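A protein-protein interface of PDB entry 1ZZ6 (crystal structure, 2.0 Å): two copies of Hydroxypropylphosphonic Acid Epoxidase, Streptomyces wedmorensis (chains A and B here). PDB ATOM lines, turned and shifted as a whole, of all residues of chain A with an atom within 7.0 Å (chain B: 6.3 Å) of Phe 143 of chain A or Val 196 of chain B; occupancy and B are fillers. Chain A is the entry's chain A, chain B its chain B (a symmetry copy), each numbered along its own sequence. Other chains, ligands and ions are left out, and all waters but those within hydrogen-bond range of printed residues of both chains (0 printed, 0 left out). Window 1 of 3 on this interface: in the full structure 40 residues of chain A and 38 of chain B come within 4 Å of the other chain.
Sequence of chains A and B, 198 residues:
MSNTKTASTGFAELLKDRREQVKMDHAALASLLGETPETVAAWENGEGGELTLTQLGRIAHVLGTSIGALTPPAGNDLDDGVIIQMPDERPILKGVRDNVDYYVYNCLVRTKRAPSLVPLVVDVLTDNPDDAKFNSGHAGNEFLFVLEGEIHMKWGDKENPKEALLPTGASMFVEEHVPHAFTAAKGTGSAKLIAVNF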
ATOM      1  N   LEU A 117      24.468   6.366  -7.088  1.00  0.00           N
ATOM      2  CA  LEU A 117      23.762   6.569  -8.353  1.00  0.00           C
ATOM      3  C   LEU A 117      23.232   7.994  -8.436  1.00  0.00           C
ATOM      4  O   LEU A 117      22.306   8.360  -7.720  1.00  0.00           O
ATOM      5  CB  LEU A 117      22.594   5.580  -8.495  1.00  0.00           C
ATOM      6  CG  LEU A 117      21.633   5.823  -9.669  1.00  0.00           C
ATOM      7  CD1 LEU A 117      22.379   5.679 -10.993  1.00  0.00           C
ATOM      8  CD2 LEU A 117      20.473   4.826  -9.612  1.00  0.00           C
ATOM      9  N   ASN A 141      33.004   6.802 -11.176  1.00  0.00           N
ATOM     10  CA  ASN A 141      32.757   6.456 -12.569  1.00  0.00           C
ATOM     11  C   ASN A 141      31.512   7.142 -13.120  1.00  0.00           C
ATOM     12  O   ASN A 141      30.584   7.473 -12.374  1.00  0.00           O
ATOM     13  CB  ASN A 141      32.629   4.939 -12.714  1.00  0.00           C
ATOM     14  CG  ASN A 141      33.941   4.223 -12.448  1.00  0.00           C
ATOM     15  OD1 ASN A 141      35.002   4.850 -12.379  1.00  0.00           O
ATOM     16  ND2 ASN A 141      33.877   2.908 -12.306  1.00  0.00           N
ATOM     17  N   GLU A 142      31.497   7.350 -14.433  1.00  0.00           N
ATOM     18  CA  GLU A 142      30.369   8.009 -15.083  1.00  0.00           C
ATOM     19  C   GLU A 142      30.112   7.461 -16.483  1.00  0.00           C
ATOM     20  O   GLU A 142      31.042   7.280 -17.266  1.00  0.00           O
ATOM     21  CB  GLU A 142      30.640   9.511 -15.182  1.00  0.00           C
ATOM     22  CG  GLU A 142      29.462  10.326 -15.683  1.00  0.00           C
ATOM     23  CD  GLU A 142      29.773  11.814 -15.762  1.00  0.00           C
ATOM     24  OE1 GLU A 142      28.818  12.622 -15.765  1.00  0.00           O
ATOM     25  OE2 GLU A 142      30.968  12.173 -15.828  1.00  0.00           O
ATOM     26  N   PHE A 143      28.848   7.183 -16.782  1.00  0.00           N
ATOM     27  CA  PHE A 143      28.456   6.694 -18.098  1.00  0.00           C
ATOM     28  C   PHE A 143      27.693   7.842 -18.732  1.00  0.00           C
ATOM     29  O   PHE A 143      26.907   8.489 -18.053  1.00  0.00           O
ATOM     30  CB  PHE A 143      27.530   5.475 -17.980  1.00  0.00           C
ATOM     31  CG  PHE A 143      26.731   5.207 -19.225  1.00  0.00           C
ATOM     32  CD1 PHE A 143      27.307   4.565 -20.312  1.00  0.00           C
ATOM     33  CD2 PHE A 143      25.418   5.666 -19.335  1.00  0.00           C
ATOM     34  CE1 PHE A 143      26.600   4.384 -21.498  1.00  0.00           C
ATOM     35  CE2 PHE A 143      24.700   5.492 -20.513  1.00  0.00           C
ATOM     36  CZ  PHE A 143      25.297   4.848 -21.600  1.00  0.00           C
ATOM     37  N   LEU A 144      27.924   8.100 -20.020  1.00  0.00           N
ATOM     38  CA  LEU A 144      27.229   9.183 -20.705  1.00  0.00           C
ATOM     39  C   LEU A 144      26.680   8.732 -22.051  1.00  0.00           C
ATOM     40  O   LEU A 144      27.221   7.825 -22.681  1.00  0.00           O
ATOM     41  CB  LEU A 144      28.155  10.393 -20.905  1.00  0.00           C
ATOM     42  CG  LEU A 144      28.631  11.093 -19.629  1.00  0.00           C
ATOM     43  CD1 LEU A 144      30.111  10.834 -19.436  1.00  0.00           C
ATOM     44  CD2 LEU A 144      28.368  12.579 -19.727  1.00  0.00           C
ATOM     45  N   PHE A 145      25.606   9.388 -22.483  1.00  0.00           N
ATOM     46  CA  PHE A 145      24.941   9.079 -23.746  1.00  0.00           C
ATOM     47  C   PHE A 145      24.533  10.411 -24.380  1.00  0.00           C
ATOM     48  O   PHE A 145      23.988  11.281 -23.709  1.00  0.00           O
ATOM     49  CB  PHE A 145      23.710   8.216 -23.445  1.00  0.00           C
ATOM     50  CG  PHE A 145      22.893   7.851 -24.654  1.00  0.00           C
ATOM     51  CD1 PHE A 145      23.308   6.846 -25.516  1.00  0.00           C
ATOM     52  CD2 PHE A 145      21.678   8.497 -24.906  1.00  0.00           C
ATOM     53  CE1 PHE A 145      22.522   6.480 -26.612  1.00  0.00           C
ATOM     54  CE2 PHE A 145      20.888   8.142 -25.994  1.00  0.00           C
ATOM     55  CZ  PHE A 145      21.310   7.131 -26.850  1.00  0.00           C
ATOM     56  N   ALA A 170      25.973   8.517 -29.431  1.00  0.00           N
ATOM     57  CA  ALA A 170      27.295   8.060 -29.035  1.00  0.00           C
ATOM     58  C   ALA A 170      27.242   7.854 -27.529  1.00  0.00           C
ATOM     59  O   ALA A 170      26.470   8.511 -26.847  1.00  0.00           O
ATOM     60  CB  ALA A 170      28.344   9.108 -29.383  1.00  0.00           C
ATOM     61  N   SER A 171      28.037   6.929 -27.013  1.00  0.00           N
ATOM     62  CA  SER A 171      28.042   6.689 -25.578  1.00  0.00           C
ATOM     63  C   SER A 171      29.484   6.673 -25.125  1.00  0.00           C
ATOM     64  O   SER A 171      30.373   6.293 -25.884  1.00  0.00           O
ATOM     65  CB  SER A 171      27.379   5.350 -25.242  1.00  0.00           C
ATOM     66  OG  SER A 171      28.136   4.250 -25.727  1.00  0.00           O
ATOM     67  N   MET A 172      29.714   7.088 -23.887  1.00  0.00           N
ATOM     68  CA  MET A 172      31.060   7.115 -23.345  1.00  0.00           C
ATOM     69  C   MET A 172      31.077   6.756 -21.864  1.00  0.00           C
ATOM     70  O   MET A 172      30.040   6.787 -21.186  1.00  0.00           O
ATOM     71  CB  MET A 172      31.678   8.507 -23.555  1.00  0.00           C
ATOM     72  CG  MET A 172      30.740   9.679 -23.286  1.00  0.00           C
ATOM     73  SD  MET A 172      29.575  10.081 -24.653  1.00  0.00           S
ATOM     74  CE  MET A 172      29.440  11.870 -24.460  1.00  0.00           C
ATOM     75  N   PHE A 173      32.259   6.376 -21.388  1.00  0.00           N
ATOM     76  CA  PHE A 173      32.488   6.045 -19.987  1.00  0.00           C
ATOM     77  C   PHE A 173      33.717   6.854 -19.589  1.00  0.00           C
ATOM     78  O   PHE A 173      34.705   6.897 -20.335  1.00  0.00           O
ATOM     79  CB  PHE A 173      32.787   4.560 -19.804  1.00  0.00           C
ATOM     80  CG  PHE A 173      33.396   4.227 -18.460  1.00  0.00           C
ATOM     81  CD1 PHE A 173      32.591   3.995 -17.352  1.00  0.00           C
ATOM     82  CD2 PHE A 173      34.782   4.195 -18.296  1.00  0.00           C
ATOM     83  CE1 PHE A 173      33.151   3.740 -16.101  1.00  0.00           C
ATOM     84  CE2 PHE A 173      35.358   3.937 -17.034  1.00  0.00           C
ATOM     85  CZ  PHE A 173      34.544   3.711 -15.943  1.00  0.00           C
ATOM     86  N   VAL A 174      33.651   7.498 -18.431  1.00  0.00           N
ATOM     87  CA  VAL A 174      34.745   8.312 -17.925  1.00  0.00           C
ATOM     88  C   VAL A 174      35.088   7.811 -16.536  1.00  0.00           C
ATOM     89  O   VAL A 174      34.215   7.702 -15.691  1.00  0.00           O
ATOM     90  CB  VAL A 174      34.330   9.781 -17.803  1.00  0.00           C
ATOM     91  CG1 VAL A 174      35.533  10.628 -17.399  1.00  0.00           C
ATOM     92  CG2 VAL A 174      33.749  10.269 -19.137  1.00  0.00           C
ATOM     93  N   ILE A 194      22.803  12.547 -21.253  1.00  0.00           N
ATOM     94  CA  ILE A 194      22.200  11.814 -20.159  1.00  0.00           C
ATOM     95  C   ILE A 194      23.470  11.308 -19.483  1.00  0.00           C
ATOM     96  O   ILE A 194      24.264  10.605 -20.103  1.00  0.00           O
ATOM     97  CB  ILE A 194      21.306  10.647 -20.651  1.00  0.00           C
ATOM     98  CG1 ILE A 194      21.219   9.561 -19.585  1.00  0.00           C
ATOM     99  CG2 ILE A 194      21.812  10.117 -21.953  1.00  0.00           C
ATOM    100  CD1 ILE A 194      20.539  10.007 -18.327  1.00  0.00           C
ATOM    101  N   ALA A 195      23.694  11.719 -18.240  1.00  0.00           N
ATOM    102  CA  ALA A 195      24.886  11.308 -17.517  1.00  0.00           C
ATOM    103  C   ALA A 195      24.514  10.450 -16.324  1.00  0.00           C
ATOM    104  O   ALA A 195      23.663  10.828 -15.522  1.00  0.00           O
ATOM    105  CB  ALA A 195      25.662  12.536 -17.054  1.00  0.00           C
ATOM    106  N   VAL A 196      25.168   9.300 -16.206  1.00  0.00           N
ATOM    107  CA  VAL A 196      24.902   8.397 -15.102  1.00  0.00           C
ATOM    108  C   VAL A 196      26.158   8.173 -14.259  1.00  0.00           C
ATOM    109  O   VAL A 196      27.077   7.443 -14.644  1.00  0.00           O
ATOM    110  CB  VAL A 196      24.377   7.048 -15.620  1.00  0.00           C
ATOM    111  CG1 VAL A 196      24.122   6.105 -14.459  1.00  0.00           C
ATOM    112  CG2 VAL A 196      23.089   7.265 -16.410  1.00  0.00           C
ATOM    113  N   ASN A 197      26.197   8.832 -13.108  1.00  0.00           N
ATOM    114  CA  ASN A 197      27.313   8.691 -12.190  1.00  0.00           C
ATOM    115  C   ASN A 197      26.920   7.550 -11.271  1.00  0.00           C
ATOM    116  O   ASN A 197      25.798   7.516 -10.775  1.00  0.00           O
ATOM    117  CB  ASN A 197      27.497   9.983 -11.385  1.00  0.00           C
ATOM    118  CG  ASN A 197      27.793  11.173 -12.272  1.00  0.00           C
ATOM    119  OD1 ASN A 197      28.947  11.441 -12.599  1.00  0.00           O
ATOM    120  ND2 ASN A 197      26.746  11.875 -12.693  1.00  0.00           N
ATOM    121  N   PHE A 198      27.833   6.601 -11.082  1.00  0.00           N
ATOM    122  CA  PHE A 198      27.598   5.460 -10.207  1.00  0.00           C
ATOM    123  C   PHE A 198      28.901   5.114  -9.486  1.00  0.00           C
ATOM    124  O   PHE A 198      29.883   5.857  -9.700  1.00  0.00           O
ATOM    125  CB  PHE A 198      27.087   4.241 -10.999  1.00  0.00           C
ATOM    126  CG  PHE A 198      28.000   3.800 -12.112  1.00  0.00           C
ATOM    127  CD1 PHE A 198      28.013   4.474 -13.328  1.00  0.00           C
ATOM    128  CD2 PHE A 198      28.856   2.707 -11.941  1.00  0.00           C
ATOM    129  CE1 PHE A 198      28.864   4.068 -14.367  1.00  0.00           C
ATOM    130  CE2 PHE A 198      29.709   2.293 -12.969  1.00  0.00           C
ATOM    131  CZ  PHE A 198      29.710   2.978 -14.186  1.00  0.00           C
ATOM    132  OXT PHE A 198      28.927   4.127  -8.713  1.00  0.00           O
ATOM    133  N   LEU B 108      25.535  -0.458 -25.749  1.00  0.00           N
ATOM    134  CA  LEU B 108      26.311   0.766 -25.729  1.00  0.00           C
ATOM    135  C   LEU B 108      27.690   0.445 -25.158  1.00  0.00           C
ATOM    136  O   LEU B 108      27.999  -0.713 -24.886  1.00  0.00           O
ATOM    137  CB  LEU B 108      25.598   1.822 -24.888  1.00  0.00           C
ATOM    138  CG  LEU B 108      24.213   2.186 -25.429  1.00  0.00           C
ATOM    139  CD1 LEU B 108      23.552   3.176 -24.505  1.00  0.00           C
ATOM    140  CD2 LEU B 108      24.366   2.773 -26.846  1.00  0.00           C
ATOM    141  N   VAL B 109      28.505   1.473 -24.962  1.00  0.00           N
ATOM    142  CA  VAL B 109      29.875   1.308 -24.496  1.00  0.00           C
ATOM    143  C   VAL B 109      30.093   0.492 -23.224  1.00  0.00           C
ATOM    144  O   VAL B 109      29.324   0.587 -22.265  1.00  0.00           O
ATOM    145  CB  VAL B 109      30.537   2.683 -24.293  1.00  0.00           C
ATOM    146  CG1 VAL B 109      30.069   3.300 -22.979  1.00  0.00           C
ATOM    147  CG2 VAL B 109      32.061   2.542 -24.327  1.00  0.00           C
ATOM    148  N   LEU B 117      29.273  -2.682 -15.797  1.00  0.00           N
ATOM    149  CA  LEU B 117      28.572  -1.682 -16.591  1.00  0.00           C
ATOM    150  C   LEU B 117      28.134  -2.277 -17.926  1.00  0.00           C
ATOM    151  O   LEU B 117      28.962  -2.588 -18.786  1.00  0.00           O
ATOM    152  CB  LEU B 117      29.459  -0.448 -16.841  1.00  0.00           C
ATOM    153  CG  LEU B 117      28.885   0.598 -17.816  1.00  0.00           C
ATOM    154  CD1 LEU B 117      27.576   1.160 -17.291  1.00  0.00           C
ATOM    155  CD2 LEU B 117      29.889   1.731 -17.994  1.00  0.00           C
ATOM    156  N   VAL B 118      26.831  -2.457 -18.086  1.00  0.00           N
ATOM    157  CA  VAL B 118      26.287  -2.977 -19.333  1.00  0.00           C
ATOM    158  C   VAL B 118      25.154  -2.051 -19.767  1.00  0.00           C
ATOM    159  O   VAL B 118      23.996  -2.264 -19.415  1.00  0.00           O
ATOM    160  CB  VAL B 118      25.705  -4.386 -19.172  1.00  0.00           C
ATOM    161  CG1 VAL B 118      25.179  -4.874 -20.521  1.00  0.00           C
ATOM    162  CG2 VAL B 118      26.767  -5.339 -18.652  1.00  0.00           C
ATOM    163  N   PRO B 119      25.476  -1.001 -20.529  1.00  0.00           N
ATOM    164  CA  PRO B 119      24.402  -0.101 -20.951  1.00  0.00           C
ATOM    165  C   PRO B 119      23.804  -0.504 -22.291  1.00  0.00           C
ATOM    166  O   PRO B 119      24.473  -1.092 -23.141  1.00  0.00           O
ATOM    167  CB  PRO B 119      25.089   1.249 -20.989  1.00  0.00           C
ATOM    168  CG  PRO B 119      26.455   0.886 -21.507  1.00  0.00           C
ATOM    169  CD  PRO B 119      26.801  -0.394 -20.761  1.00  0.00           C
ATOM    170  N   LEU B 120      22.536  -0.173 -22.479  1.00  0.00           N
ATOM    171  CA  LEU B 120      21.857  -0.540 -23.714  1.00  0.00           C
ATOM    172  C   LEU B 120      20.739   0.412 -24.058  1.00  0.00           C
ATOM    173  O   LEU B 120      20.248   1.155 -23.204  1.00  0.00           O
ATOM    174  CB  LEU B 120      21.197  -1.915 -23.564  1.00  0.00           C
ATOM    175  CG  LEU B 120      21.860  -3.009 -22.738  1.00  0.00           C
ATOM    176  CD1 LEU B 120      20.793  -4.013 -22.296  1.00  0.00           C
ATOM    177  CD2 LEU B 120      22.949  -3.678 -23.557  1.00  0.00           C
ATOM    178  N   ASN B 141      22.027  -4.081  -9.965  1.00  0.00           N
ATOM    179  CA  ASN B 141      21.197  -2.880 -10.004  1.00  0.00           C
ATOM    180  C   ASN B 141      21.057  -2.374 -11.434  1.00  0.00           C
ATOM    181  O   ASN B 141      21.898  -2.653 -12.294  1.00  0.00           O
ATOM    182  CB  ASN B 141      21.797  -1.763  -9.147  1.00  0.00           C
ATOM    183  CG  ASN B 141      21.758  -2.075  -7.657  1.00  0.00           C
ATOM    184  OD1 ASN B 141      20.860  -2.766  -7.170  1.00  0.00           O
ATOM    185  ND2 ASN B 141      22.726  -1.538  -6.923  1.00  0.00           N
ATOM    186  N   GLU B 142      20.004  -1.607 -11.676  1.00  0.00           N
ATOM    187  CA  GLU B 142      19.753  -1.086 -13.007  1.00  0.00           C
ATOM    188  C   GLU B 142      19.007   0.245 -12.972  1.00  0.00           C
ATOM    189  O   GLU B 142      18.091   0.442 -12.177  1.00  0.00           O
ATOM    190  CB  GLU B 142      18.964  -2.126 -13.807  1.00  0.00           C
ATOM    191  CG  GLU B 142      18.590  -1.701 -15.212  1.00  0.00           C
ATOM    192  CD  GLU B 142      17.921  -2.811 -16.007  1.00  0.00           C
ATOM    193  OE1 GLU B 142      17.002  -3.465 -15.470  1.00  0.00           O
ATOM    194  OE2 GLU B 142      18.306  -3.024 -17.176  1.00  0.00           O
ATOM    195  N   PHE B 143      19.433   1.161 -13.831  1.00  0.00           N
ATOM    196  CA  PHE B 143      18.811   2.464 -13.952  1.00  0.00           C
ATOM    197  C   PHE B 143      18.193   2.501 -15.344  1.00  0.00           C
ATOM    198  O   PHE B 143      18.791   2.014 -16.310  1.00  0.00           O
ATOM    199  CB  PHE B 143      19.853   3.569 -13.827  1.00  0.00           C
ATOM    200  CG  PHE B 143      19.409   4.875 -14.406  1.00  0.00           C
ATOM    201  CD1 PHE B 143      18.544   5.702 -13.702  1.00  0.00           C
ATOM    202  CD2 PHE B 143      19.814   5.253 -15.688  1.00  0.00           C
ATOM    203  CE1 PHE B 143      18.085   6.889 -14.258  1.00  0.00           C
ATOM    204  CE2 PHE B 143      19.358   6.433 -16.253  1.00  0.00           C
ATOM    205  CZ  PHE B 143      18.489   7.254 -15.537  1.00  0.00           C
ATOM    206  N   LEU B 144      16.996   3.058 -15.454  1.00  0.00           N
ATOM    207  CA  LEU B 144      16.344   3.128 -16.754  1.00  0.00           C
ATOM    208  C   LEU B 144      15.774   4.507 -17.011  1.00  0.00           C
ATOM    209  O   LEU B 144      15.487   5.258 -16.082  1.00  0.00           O
ATOM    210  CB  LEU B 144      15.240   2.073 -16.864  1.00  0.00           C
ATOM    211  CG  LEU B 144      15.735   0.641 -16.680  1.00  0.00           C
ATOM    212  CD1 LEU B 144      15.369   0.167 -15.292  1.00  0.00           C
ATOM    213  CD2 LEU B 144      15.132  -0.274 -17.734  1.00  0.00           C
ATOM    214  N   ILE B 194      16.590   3.544 -22.226  1.00  0.00           N
ATOM    215  CA  ILE B 194      18.012   3.383 -21.994  1.00  0.00           C
ATOM    216  C   ILE B 194      18.056   2.601 -20.691  1.00  0.00           C
ATOM    217  O   ILE B 194      17.399   2.954 -19.716  1.00  0.00           O
ATOM    218  CB  ILE B 194      18.733   4.722 -21.794  1.00  0.00           C
ATOM    219  CG1 ILE B 194      18.738   5.515 -23.098  1.00  0.00           C
ATOM    220  CG2 ILE B 194      20.192   4.469 -21.372  1.00  0.00           C
ATOM    221  CD1 ILE B 194      19.197   6.965 -22.929  1.00  0.00           C
ATOM    222  N   ALA B 195      18.796   1.507 -20.699  1.00  0.00           N
ATOM    223  CA  ALA B 195      18.919   0.679 -19.525  1.00  0.00           C
ATOM    224  C   ALA B 195      20.399   0.621 -19.196  1.00  0.00           C
ATOM    225  O   ALA B 195      21.202   0.214 -20.027  1.00  0.00           O
ATOM    226  CB  ALA B 195      18.383  -0.715 -19.818  1.00  0.00           C
ATOM    227  N   VAL B 196      20.753   1.051 -17.992  1.00  0.00           N
ATOM    228  CA  VAL B 196      22.140   1.024 -17.570  1.00  0.00           C
ATOM    229  C   VAL B 196      22.273   0.085 -16.391  1.00  0.00           C
ATOM    230  O   VAL B 196      21.873   0.421 -15.286  1.00  0.00           O
ATOM    231  CB  VAL B 196      22.642   2.411 -17.125  1.00  0.00           C
ATOM    232  CG1 VAL B 196      24.101   2.307 -16.697  1.00  0.00           C
ATOM    233  CG2 VAL B 196      22.495   3.422 -18.258  1.00  0.00           C
ATOM    234  N   ASN B 197      22.814  -1.103 -16.639  1.00  0.00           N
ATOM    235  CA  ASN B 197      23.037  -2.076 -15.582  1.00  0.00           C
ATOM    236  C   ASN B 197      24.392  -1.711 -14.980  1.00  0.00           C
ATOM    237  O   ASN B 197      25.291  -1.282 -15.697  1.00  0.00           O
ATOM    238  CB  ASN B 197      23.068  -3.484 -16.173  1.00  0.00           C
ATOM    239  CG  ASN B 197      21.709  -3.921 -16.712  1.00  0.00           C
ATOM    240  OD1 ASN B 197      20.825  -4.318 -15.951  1.00  0.00           O
ATOM    241  ND2 ASN B 197      21.535  -3.832 -18.028  1.00  0.00           N
ATOM    242  N   PHE B 198      24.536  -1.846 -13.668  1.00  0.00           N
ATOM    243  CA  PHE B 198      25.802  -1.508 -13.022  1.00  0.00           C
ATOM    244  C   PHE B 198      25.927  -2.160 -11.647  1.00  0.00           C
ATOM    245  O   PHE B 198      24.931  -2.758 -11.190  1.00  0.00           O
ATOM    246  CB  PHE B 198      25.938   0.010 -12.871  1.00  0.00           C
ATOM    247  CG  PHE B 198      24.959   0.621 -11.901  1.00  0.00           C
ATOM    248  CD1 PHE B 198      23.622   0.796 -12.249  1.00  0.00           C
ATOM    249  CD2 PHE B 198      25.378   1.017 -10.632  1.00  0.00           C
ATOM    250  CE1 PHE B 198      22.714   1.356 -11.346  1.00  0.00           C
ATOM    251  CE2 PHE B 198      24.479   1.578  -9.724  1.00  0.00           C
ATOM    252  CZ  PHE B 198      23.145   1.746 -10.085  1.00  0.00           C
ATOM    253  OXT PHE B 198      27.019  -2.055 -11.041  1.00  0.00           O
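The backbone carbonyl oxygen (O) of Asn 141 of chain A lies within hydrogen-bond range of the backbone NH (N) of Phe 198 of chain A (3.2 Å).
The backbone carbonyl oxygen (O) of Phe 143 of chain A is in hydrogen-bond range of the backbone NH (N) of Val 196 of chain A, 2.7 Å away.
N of Leu 144 of chain A is in hydrogen-bond range of O of Met 172 of chain A (2.7 Å).
N of Leu 108 of chain B sits at hydrogen-bond distance from O of Pro 119 of chain B, at 2.9 Å.
The backbone carbonyl oxygen of Asn 141 of chain B is in hydrogen-bond range of the backbone NH of Phe 198 of chain B (3.1 Å).
The backbone carbonyl oxygen (O) of Phe 143 of chain B sits at hydrogen-bond distance from the backbone NH (N) of Val 196 of chain B (2.8 Å).
Of chain B, only Leu 108 (3.8 Å), Val 109 (3.9 Å), Pro 119 (3.5 Å) and Val 196 (3.8 Å) come within 4 Å of Phe 143 of chain A.
Printed residues of chain A within 4 Å of Val 196 of chain B: Phe 143.
Of the printed residues of chain A, Pro 119 of chain B touches Phe 143.
Of the printed residues of chain A, Phe 143 of chain B touches Val 196 (3.8 Å).
The nearest residue of chain B that does not touch Phe 143 of chain A is Leu 117 of chain B (4.4 Å).
The nearest printed residue of chain A that does not touch Ile 194 of chain B is Ile 194 of chain A (4.2 Å).
Phe 143 of chain A touches Val 196 of chain B, and with the chains exchanged Val 196 of chain A touches Phe 143 of chain B.
Phe 198 of chain A touches its own counterpart, Phe 198 of chain B.
Of the 12 pairs that touch across the chains among the printed residues, 3 have their exchanged pair printed and touching as well.
Of the 16 printed residues of chain A, 7 touch a printed residue of chain B.
Among the printed residues, 12 pairs touch across the chains.
Among the printed residues, no Asp or Glu carboxylate lies within 4 Å of a Lys or Arg side-chain nitrogen of the other chain.
Among the printed residues, pairs that only touch across the chains: Phe 143 of chain A with Pro 119 of chain B, Phe 145 of chain A with Ile 194 of chain B, Phe 173 of chain A with Leu 117 of chain B, Ser 171 of chain A with Leu 108 of chain B, Phe 198 of chain A with Phe 198 of chain B, Met 172 of chain A with Val 109 of chain B, Phe 143 of chain A with Val 196 of chain B, Phe 143 of chain A with Leu 108 of chain B, Phe 145 of chain A with Leu 108 of chain B, Val 196 of chain A with Phe 143 of chain B and Phe 143 of chain A with Val 109 of chain B.
OG of Ser 171 of chain A sits at hydrogen-bond distance from N of Val 109 of chain B.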
